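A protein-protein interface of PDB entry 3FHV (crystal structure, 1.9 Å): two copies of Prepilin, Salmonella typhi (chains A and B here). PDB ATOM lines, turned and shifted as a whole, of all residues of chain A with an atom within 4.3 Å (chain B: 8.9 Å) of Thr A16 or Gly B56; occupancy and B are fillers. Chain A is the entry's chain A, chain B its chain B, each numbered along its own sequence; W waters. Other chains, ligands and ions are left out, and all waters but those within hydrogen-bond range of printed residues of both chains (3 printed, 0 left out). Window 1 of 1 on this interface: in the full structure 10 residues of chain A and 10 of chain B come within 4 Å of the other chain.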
ATOM      1  N   THR A  12       1.868  11.755 -11.657  1.00  0.00           N
ATOM      2  CA  THR A  12       2.050  11.907 -10.224  1.00  0.00           C
ATOM      3  C   THR A  12       1.600  10.647  -9.484  1.00  0.00           C
ATOM      4  O   THR A  12       2.202  10.262  -8.474  1.00  0.00           O
ATOM      5  CB  THR A  12       1.254  13.122  -9.704  1.00  0.00           C
ATOM      6  OG1 THR A  12       1.721  14.298 -10.376  1.00  0.00           O
ATOM      7  CG2 THR A  12       1.443  13.293  -8.185  1.00  0.00           C
ATOM      8  N   ASN A  13       0.546  10.007  -9.986  1.00  0.00           N
ATOM      9  CA  ASN A  13       0.032   8.796  -9.350  1.00  0.00           C
ATOM     10  C   ASN A  13       1.042   7.662  -9.406  1.00  0.00           C
ATOM     11  O   ASN A  13       1.268   6.982  -8.407  1.00  0.00           O
ATOM     12  CB  ASN A  13      -1.294   8.345  -9.994  1.00  0.00           C
ATOM     13  CG  ASN A  13      -2.496   9.105  -9.451  1.00  0.00           C
ATOM     14  OD1 ASN A  13      -2.466   9.607  -8.328  1.00  0.00           O
ATOM     15  ND2 ASN A  13      -3.568   9.163 -10.234  1.00  0.00           N
ATOM     16  N   TYR A  14       1.657   7.454 -10.569  1.00  0.00           N
ATOM     17  CA  TYR A  14       2.637   6.381 -10.691  1.00  0.00           C
ATOM     18  C   TYR A  14       3.888   6.691  -9.881  1.00  0.00           C
ATOM     19  O   TYR A  14       4.466   5.808  -9.261  1.00  0.00           O
ATOM     20  CB  TYR A  14       3.016   6.156 -12.161  1.00  0.00           C
ATOM     21  CG  TYR A  14       1.834   5.750 -13.013  1.00  0.00           C
ATOM     22  CD1 TYR A  14       0.988   4.711 -12.614  1.00  0.00           C
ATOM     23  CD2 TYR A  14       1.534   6.433 -14.189  1.00  0.00           C
ATOM     24  CE1 TYR A  14      -0.142   4.372 -13.368  1.00  0.00           C
ATOM     25  CE2 TYR A  14       0.416   6.102 -14.944  1.00  0.00           C
ATOM     26  CZ  TYR A  14      -0.419   5.080 -14.527  1.00  0.00           C
ATOM     27  OH  TYR A  14      -1.543   4.782 -15.252  1.00  0.00           O
ATOM     28  N   GLN A  15       4.305   7.951  -9.882  1.00  0.00           N
ATOM     29  CA  GLN A  15       5.504   8.327  -9.151  1.00  0.00           C
ATOM     30  C   GLN A  15       5.322   8.136  -7.650  1.00  0.00           C
ATOM     31  O   GLN A  15       6.203   7.582  -6.980  1.00  0.00           O
ATOM     32  CB  GLN A  15       5.896   9.776  -9.484  1.00  0.00           C
ATOM     33  CG  GLN A  15       6.471   9.924 -10.894  1.00  0.00           C
ATOM     34  CD  GLN A  15       6.668  11.371 -11.311  1.00  0.00           C
ATOM     35  OE1 GLN A  15       6.670  12.267 -10.480  1.00  0.00           O
ATOM     36  NE2 GLN A  15       6.840  11.601 -12.610  1.00  0.00           N
ATOM     37  N   THR A  16       4.179   8.571  -7.127  1.00  0.00           N
ATOM     38  CA  THR A  16       3.917   8.427  -5.702  1.00  0.00           C
ATOM     39  C   THR A  16       3.686   6.968  -5.315  1.00  0.00           C
ATOM     40  O   THR A  16       4.116   6.540  -4.245  1.00  0.00           O
ATOM     41  CB  THR A  16       2.708   9.298  -5.243  1.00  0.00           C
ATOM     42  OG1 THR A  16       1.571   9.046  -6.073  1.00  0.00           O
ATOM     43  CG2 THR A  16       3.054  10.778  -5.315  1.00  0.00           C
ATOM     44  N   LEU A  17       3.003   6.211  -6.178  1.00  0.00           N
ATOM     45  CA  LEU A  17       2.751   4.796  -5.917  1.00  0.00           C
ATOM     46  C   LEU A  17       4.105   4.093  -5.799  1.00  0.00           C
ATOM     47  O   LEU A  17       4.303   3.249  -4.923  1.00  0.00           O
ATOM     48  CB  LEU A  17       1.919   4.165  -7.052  1.00  0.00           C
ATOM     49  CG  LEU A  17       1.625   2.658  -6.950  1.00  0.00           C
ATOM     50  CD1 LEU A  17       0.870   2.356  -5.664  1.00  0.00           C
ATOM     51  CD2 LEU A  17       0.834   2.199  -8.169  1.00  0.00           C
ATOM     52  N   ALA A  18       5.041   4.459  -6.667  1.00  0.00           N
ATOM     53  CA  ALA A  18       6.381   3.873  -6.629  1.00  0.00           C
ATOM     54  C   ALA A  18       7.066   4.232  -5.309  1.00  0.00           C
ATOM     55  O   ALA A  18       7.632   3.369  -4.645  1.00  0.00           O
ATOM     56  CB  ALA A  18       7.219   4.382  -7.811  1.00  0.00           C
ATOM     57  N   THR A  19       7.011   5.508  -4.933  1.00  0.00           N
ATOM     58  CA  THR A  19       7.622   5.953  -3.688  1.00  0.00           C
ATOM     59  C   THR A  19       7.028   5.213  -2.484  1.00  0.00           C
ATOM     60  O   THR A  19       7.764   4.765  -1.600  1.00  0.00           O
ATOM     61  CB  THR A  19       7.452   7.479  -3.514  1.00  0.00           C
ATOM     62  OG1 THR A  19       8.236   8.150  -4.509  1.00  0.00           O
ATOM     63  CG2 THR A  19       7.908   7.920  -2.115  1.00  0.00           C
ATOM     64  N   ASN A  20       5.702   5.071  -2.463  1.00  0.00           N
ATOM     65  CA  ASN A  20       5.031   4.367  -1.378  1.00  0.00           C
ATOM     66  C   ASN A  20       5.442   2.901  -1.340  1.00  0.00           C
ATOM     67  O   ASN A  20       5.648   2.332  -0.272  1.00  0.00           O
ATOM     68  CB  ASN A  20       3.512   4.461  -1.524  1.00  0.00           C
ATOM     69  CG  ASN A  20       2.999   5.872  -1.330  1.00  0.00           C
ATOM     70  OD1 ASN A  20       3.597   6.658  -0.599  1.00  0.00           O
ATOM     71  ND2 ASN A  20       1.884   6.191  -1.966  1.00  0.00           N
ATOM     72  N   GLY A  51      -4.978   8.552  -5.076  1.00  0.00           N
ATOM     73  CA  GLY A  51      -5.362   9.253  -6.295  1.00  0.00           C
ATOM     74  C   GLY A  51      -5.862   8.407  -7.456  1.00  0.00           C
ATOM     75  O   GLY A  51      -6.315   8.950  -8.465  1.00  0.00           O
ATOM     76  N   ASP B  41       2.456  20.152  -3.070  1.00  0.00           N
ATOM     77  CA  ASP B  41       3.127  19.447  -4.160  1.00  0.00           C
ATOM     78  C   ASP B  41       4.623  19.782  -4.177  1.00  0.00           C
ATOM     79  O   ASP B  41       5.479  18.897  -4.307  1.00  0.00           O
ATOM     80  CB  ASP B  41       2.532  19.859  -5.502  1.00  0.00           C
ATOM     81  CG  ASP B  41       3.295  19.273  -6.670  1.00  0.00           C
ATOM     82  OD1 ASP B  41       3.146  18.060  -6.919  1.00  0.00           O
ATOM     83  OD2 ASP B  41       4.055  20.017  -7.323  1.00  0.00           O
ATOM     84  N   ILE B  44       6.465  18.160  -1.383  1.00  0.00           N
ATOM     85  CA  ILE B  44       6.675  16.750  -1.682  1.00  0.00           C
ATOM     86  C   ILE B  44       7.803  16.584  -2.701  1.00  0.00           C
ATOM     87  O   ILE B  44       8.678  15.729  -2.540  1.00  0.00           O
ATOM     88  CB  ILE B  44       5.370  16.094  -2.208  1.00  0.00           C
ATOM     89  CG1 ILE B  44       4.369  15.975  -1.050  1.00  0.00           C
ATOM     90  CG2 ILE B  44       5.656  14.704  -2.780  1.00  0.00           C
ATOM     91  CD1 ILE B  44       2.961  15.577  -1.481  1.00  0.00           C
ATOM     92  N   GLN B  45       7.800  17.412  -3.740  1.00  0.00           N
ATOM     93  CA  GLN B  45       8.850  17.328  -4.756  1.00  0.00           C
ATOM     94  C   GLN B  45      10.220  17.640  -4.149  1.00  0.00           C
ATOM     95  O   GLN B  45      11.251  17.174  -4.641  1.00  0.00           O
ATOM     96  CB  GLN B  45       8.572  18.301  -5.903  1.00  0.00           C
ATOM     97  CG  GLN B  45       7.190  18.173  -6.526  1.00  0.00           C
ATOM     98  CD  GLN B  45       6.898  16.790  -7.069  1.00  0.00           C
ATOM     99  OE1 GLN B  45       5.748  16.464  -7.374  1.00  0.00           O
ATOM    100  NE2 GLN B  45       7.934  15.967  -7.201  1.00  0.00           N
ATOM    101  N   LYS B  50       9.210  12.455   2.576  1.00  0.00           N
ATOM    102  CA  LYS B  50       9.667  11.077   2.437  1.00  0.00           C
ATOM    103  C   LYS B  50       9.340  10.322   3.715  1.00  0.00           C
ATOM    104  O   LYS B  50       9.611  10.809   4.810  1.00  0.00           O
ATOM    105  CB  LYS B  50      11.174  11.027   2.181  1.00  0.00           C
ATOM    106  CG  LYS B  50      11.602  11.604   0.845  1.00  0.00           C
ATOM    107  CD  LYS B  50      11.080  10.781  -0.311  1.00  0.00           C
ATOM    108  CE  LYS B  50      11.446  11.425  -1.635  1.00  0.00           C
ATOM    109  NZ  LYS B  50      10.893  10.672  -2.794  1.00  0.00           N
ATOM    110  N   MET B  52       6.244   9.418   4.432  1.00  0.00           N
ATOM    111  CA  MET B  52       4.809   9.586   4.605  1.00  0.00           C
ATOM    112  C   MET B  52       4.126   9.182   3.304  1.00  0.00           C
ATOM    113  O   MET B  52       4.739   9.225   2.233  1.00  0.00           O
ATOM    114  CB  MET B  52       4.475  11.040   4.952  1.00  0.00           C
ATOM    115  CG  MET B  52       4.992  11.487   6.315  1.00  0.00           C
ATOM    116  SD  MET B  52       4.552  13.201   6.698  1.00  0.00           S
ATOM    117  CE  MET B  52       2.918  12.997   7.192  1.00  0.00           C
ATOM    118  N   THR B  53       2.862   8.787   3.387  1.00  0.00           N
ATOM    119  CA  THR B  53       2.133   8.371   2.197  1.00  0.00           C
ATOM    120  C   THR B  53       1.738   9.557   1.329  1.00  0.00           C
ATOM    121  O   THR B  53       1.188  10.545   1.811  1.00  0.00           O
ATOM    122  CB  THR B  53       0.863   7.579   2.558  1.00  0.00           C
ATOM    123  OG1 THR B  53       1.227   6.438   3.343  1.00  0.00           O
ATOM    124  CG2 THR B  53       0.160   7.098   1.285  1.00  0.00           C
ATOM    125  N   VAL B  54       2.030   9.438   0.042  1.00  0.00           N
ATOM    126  CA  VAL B  54       1.725  10.475  -0.919  1.00  0.00           C
ATOM    127  C   VAL B  54       0.925   9.915  -2.095  1.00  0.00           C
ATOM    128  O   VAL B  54       0.912   8.704  -2.332  1.00  0.00           O
ATOM    129  CB  VAL B  54       3.034  11.116  -1.436  1.00  0.00           C
ATOM    130  CG1 VAL B  54       3.661  11.975  -0.326  1.00  0.00           C
ATOM    131  CG2 VAL B  54       4.028  10.020  -1.844  1.00  0.00           C
ATOM    132  N   SER B  55       0.236  10.792  -2.815  1.00  0.00           N
ATOM    133  CA  SER B  55      -0.520  10.366  -3.981  1.00  0.00           C
ATOM    134  C   SER B  55      -0.698  11.538  -4.937  1.00  0.00           C
ATOM    135  O   SER B  55      -0.025  12.557  -4.799  1.00  0.00           O
ATOM    136  CB  SER B  55      -1.878   9.786  -3.576  1.00  0.00           C
ATOM    137  OG  SER B  55      -2.357   8.926  -4.601  1.00  0.00           O
ATOM    138  N   GLY B  56      -1.583  11.384  -5.918  1.00  0.00           N
ATOM    139  CA  GLY B  56      -1.809  12.439  -6.887  1.00  0.00           C
ATOM    140  C   GLY B  56      -3.229  12.979  -6.865  1.00  0.00           C
ATOM    141  O   GLY B  56      -4.194  12.233  -6.710  1.00  0.00           O
ATOM    142  N   ASP B  57      -3.354  14.287  -7.039  1.00  0.00           N
ATOM    143  CA  ASP B  57      -4.653  14.945  -7.027  1.00  0.00           C
ATOM    144  C   ASP B  57      -5.251  14.995  -8.426  1.00  0.00           C
ATOM    145  O   ASP B  57      -4.691  15.613  -9.317  1.00  0.00           O
ATOM    146  CB  ASP B  57      -4.500  16.367  -6.470  1.00  0.00           C
ATOM    147  CG  ASP B  57      -5.756  17.206  -6.640  1.00  0.00           C
ATOM    148  OD1 ASP B  57      -6.869  16.650  -6.569  1.00  0.00           O
ATOM    149  OD2 ASP B  57      -5.622  18.430  -6.835  1.00  0.00           O
ATOM    150  N   PRO B  58      -6.402  14.332  -8.631  1.00  0.00           N
ATOM    151  CA  PRO B  58      -7.076  14.306  -9.935  1.00  0.00           C
ATOM    152  C   PRO B  58      -7.466  15.691 -10.437  1.00  0.00           C
ATOM    153  O   PRO B  58      -7.608  15.906 -11.640  1.00  0.00           O
ATOM    154  CB  PRO B  58      -8.305  13.434  -9.674  1.00  0.00           C
ATOM    155  CG  PRO B  58      -7.851  12.527  -8.578  1.00  0.00           C
ATOM    156  CD  PRO B  58      -7.104  13.467  -7.666  1.00  0.00           C
ATOM    157  N   ALA B  59      -7.640  16.634  -9.518  1.00  0.00           N
ATOM    158  CA  ALA B  59      -8.029  17.987  -9.906  1.00  0.00           C
ATOM    159  C   ALA B  59      -6.884  18.825 -10.467  1.00  0.00           C
ATOM    160  O   ALA B  59      -7.009  19.426 -11.532  1.00  0.00           O
ATOM    161  CB  ALA B  59      -8.659  18.713  -8.714  1.00  0.00           C
ATOM    162  N   SER B  60      -5.764  18.856  -9.755  1.00  0.00           N
ATOM    163  CA  SER B  60      -4.626  19.669 -10.170  1.00  0.00           C
ATOM    164  C   SER B  60      -3.430  18.911 -10.722  1.00  0.00           C
ATOM    165  O   SER B  60      -2.568  19.510 -11.360  1.00  0.00           O
ATOM    166  CB  SER B  60      -4.142  20.492  -8.985  1.00  0.00           C
ATOM    167  OG  SER B  60      -3.645  19.617  -7.988  1.00  0.00           O
ATOM    168  N   GLY B  61      -3.361  17.610 -10.465  1.00  0.00           N
ATOM    169  CA  GLY B  61      -2.218  16.844 -10.925  1.00  0.00           C
ATOM    170  C   GLY B  61      -1.069  16.968  -9.928  1.00  0.00           C
ATOM    171  O   GLY B  61       0.001  16.400 -10.123  1.00  0.00           O
ATOM    172  N   SER B  62      -1.289  17.722  -8.853  1.00  0.00           N
ATOM    173  CA  SER B  62      -0.268  17.905  -7.817  1.00  0.00           C
ATOM    174  C   SER B  62      -0.204  16.710  -6.860  1.00  0.00           C
ATOM    175  O   SER B  62      -1.187  15.996  -6.690  1.00  0.00           O
ATOM    176  CB  SER B  62      -0.561  19.168  -7.007  1.00  0.00           C
ATOM    177  OG  SER B  62      -0.392  20.322  -7.803  1.00  0.00           O
ATOM    178  N   ALA B  63       0.952  16.500  -6.233  1.00  0.00           N
ATOM    179  CA  ALA B  63       1.106  15.400  -5.287  1.00  0.00           C
ATOM    180  C   ALA B  63       0.380  15.776  -3.999  1.00  0.00           C
ATOM    181  O   ALA B  63       0.379  16.940  -3.597  1.00  0.00           O
ATOM    182  CB  ALA B  63       2.592  15.140  -5.004  1.00  0.00           C
ATOM    183  N   THR B  64      -0.247  14.785  -3.372  1.00  0.00           N
ATOM    184  CA  THR B  64      -0.986  14.983  -2.133  1.00  0.00           C
ATOM    185  C   THR B  64      -0.325  14.232  -0.984  1.00  0.00           C
ATOM    186  O   THR B  64       0.396  13.254  -1.199  1.00  0.00           O
ATOM    187  CB  THR B  64      -2.445  14.510  -2.271  1.00  0.00           C
ATOM    188  OG1 THR B  64      -2.466  13.150  -2.729  1.00  0.00           O
ATOM    189  CG2 THR B  64      -3.200  15.401  -3.267  1.00  0.00           C
ATOM    190  N   LEU B  65      -0.571  14.695   0.237  1.00  0.00           N
ATOM    191  CA  LEU B  65       0.046  14.105   1.419  1.00  0.00           C
ATOM    192  C   LEU B  65      -1.009  13.623   2.410  1.00  0.00           C
ATOM    193  O   LEU B  65      -2.096  14.191   2.498  1.00  0.00           O
ATOM    194  CB  LEU B  65       0.981  15.111   2.093  1.00  0.00           C
ATOM    195  CG  LEU B  65       1.646  14.653   3.393  1.00  0.00           C
ATOM    196  CD1 LEU B  65       2.705  13.598   3.112  1.00  0.00           C
ATOM    197  CD2 LEU B  65       2.246  15.836   4.137  1.00  0.00           C
ATOM    198  N   TRP B  66      -0.678  12.573   3.153  1.00  0.00           N
ATOM    199  CA  TRP B  66      -1.683  11.791   3.865  1.00  0.00           C
ATOM    200  C   TRP B  66      -1.152  11.303   5.208  1.00  0.00           C
ATOM    201  O   TRP B  66      -0.074  10.714   5.284  1.00  0.00           O
ATOM    202  CB  TRP B  66      -2.136  10.603   3.016  1.00  0.00           C
ATOM    203  CG  TRP B  66      -2.751  10.998   1.709  1.00  0.00           C
ATOM    204  CD1 TRP B  66      -2.127  11.067   0.497  1.00  0.00           C
ATOM    205  CD2 TRP B  66      -4.113  11.381   1.481  1.00  0.00           C
ATOM    206  NE1 TRP B  66      -3.016  11.469  -0.470  1.00  0.00           N
ATOM    207  CE2 TRP B  66      -4.241  11.668   0.107  1.00  0.00           C
ATOM    208  CE3 TRP B  66      -5.235  11.509   2.305  1.00  0.00           C
ATOM    209  CZ2 TRP B  66      -5.446  12.075  -0.460  1.00  0.00           C
ATOM    210  CZ3 TRP B  66      -6.431  11.913   1.739  1.00  0.00           C
ATOM    211  CH2 TRP B  66      -6.528  12.191   0.370  1.00  0.00           C
ATOM    212  N   GLN B  72      -6.237  13.548   5.171  1.00  0.00           N
ATOM    213  CA  GLN B  72      -5.306  14.275   4.328  1.00  0.00           C
ATOM    214  C   GLN B  72      -4.542  15.310   5.152  1.00  0.00           C
ATOM    215  O   GLN B  72      -4.988  15.727   6.230  1.00  0.00           O
ATOM    216  CB  GLN B  72      -6.059  14.968   3.190  1.00  0.00           C
ATOM    217  CG  GLN B  72      -5.172  15.653   2.167  1.00  0.00           C
ATOM    218  CD  GLN B  72      -5.958  16.136   0.956  1.00  0.00           C
ATOM    219  OE1 GLN B  72      -7.186  16.246   1.008  1.00  0.00           O
ATOM    220  NE2 GLN B  72      -5.253  16.438  -0.136  1.00  0.00           N
HETATM  221  O   HOH W   1      -0.253   6.937  -5.268  1.00  0.00           O
HETATM  222  O   HOH W   2       3.107  17.389  -9.635  1.00  0.00           O
HETATM  223  O   HOH W   3       8.627  13.930  -9.614  1.00  0.00           O
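Among the printed residues, pairs that only touch across the chains: Gly A51 with Gly B56 (3.2 Å), Thr A16 with Ser B55 (3.2 Å), Thr A16 with Val B54 (3.5 Å), Asn A20 with Thr B53 (3.6 Å), Thr A12 with Ala B63 (3.6 Å), Thr A12 with Gly B56 (3.6 Å), Thr A12 with Ser B55 (3.8 Å), Asn A13 with Ser B55 (3.8 Å), Gly A51 with Pro B58 (3.9 Å), Thr A16 with Gly B56 (3.9 Å) and Asn A20 with Met B52 (3.99 Å).
Water W3 bridges OE1 of Gln A15 (2.7 Å) and NE2 of Gln B45 (3.2 Å).
Water W2 lies within hydrogen-bond range of OD1 of Asp B41 (2.8 Å), O of Gly B61 (3.3 Å) and OG1 of Thr A12 (3.5 Å).
Water W1 lies within hydrogen-bond range of OG1 of Thr A16 (2.9 Å), OG of Ser B55 (3.0 Å), N of Leu A17 (3.5 Å) and O of Asn A13 (3.5 Å).
No position is printed for both chains.
Of the 15 pairs that touch across the chains among the printed residues, none has its exchanged pair printed and touching as well.
Of the 20 printed residues of chain B, 8 touch a printed residue of chain A.
Hydrophobic or aromatic side chains of chain B that line the printed part of chain A: Val B54, Pro B58 and Ala B63.
Of the 10 printed residues of chain A, 5 touch a printed residue of chain B.
Among the printed residues, 15 pairs touch across the chains.
Among the printed residues, no Asp or Glu carboxylate lies within 4 Å of a Lys or Arg side-chain nitrogen of the other chain.
Thr A16 touches three residues of chain B.
Gly B56 touches just these residues of chain A: Thr A12 (3.6 Å), Asn A13 (3.1 Å), Thr A16 (3.9 Å) and Gly A51 (3.2 Å).
Thr A19 touches none of the printed residues of chain B.
Of chain B, only Ser B55, Gly B56 and Pro B58 come within 4 Å of Gly A51.
Of the printed residues of chain A, Met B52 touches Asn A20 (3.99 Å).
Printed residues of chain B within 4 Å of Asn A13: Ser B55 and Gly B56.
Printed residues of chain A within 4 Å of Ser B55: Thr A12 (3.8 Å), Asn A13 (3.8 Å), Thr A16 (3.2 Å) and Gly A51 (2.7 Å).
Printed residues of chain B within 4 Å of Thr A12: Ser B55 (3.8 Å), Gly B56 (3.6 Å), Gly B61 (2.7 Å) and Ala B63 (3.6 Å).
Ser B60 touches none of the printed residues of chain A.
Gln B72 touches none of the printed residues of chain A.
The nearest residue of chain B that does not touch Thr A16 is Ala B63 (4.4 Å).
The nearest printed residue of chain A that does not touch Thr B53 is Thr A16 (6.6 Å).
O of Val B54 lies within hydrogen-bond range of ND2 of Asn A20.
The backbone NH (N) of Gly B56 lies within hydrogen-bond range of the side-chain amide oxygen (OD1) of Asn A13 (3.1 Å).
The backbone carbonyl oxygen (O) of Gly B61 is in hydrogen-bond range of the side-chain hydroxyl (OG1) of Thr A12 (2.7 Å).
OG of Ser B55 lies within hydrogen-bond range of N of Gly A51 (2.7 Å).
The backbone NH (N) of Ala B63 is in hydrogen-bond range of the side-chain carboxylate (OD1) of Asp B41 (2.8 Å).
O of Thr B53 lies within hydrogen-bond range of N of Trp B66, 3.1 Å away.
The backbone carbonyl oxygen of Ser B55 sits at hydrogen-bond distance from the backbone NH of Thr B64, 2.7 Å away.
The side-chain amide nitrogen (ND2) of Asn A13 lies within hydrogen-bond range of the backbone carbonyl oxygen (O) of Gly A51.
The backbone carbonyl oxygen (O) of Thr A16 lies close to the side-chain amide nitrogen (ND2) of Asn A20 (3.2 Å).
O of Asn A13 sits at hydrogen-bond distance from OG1 of Thr A16 (3.1 Å).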
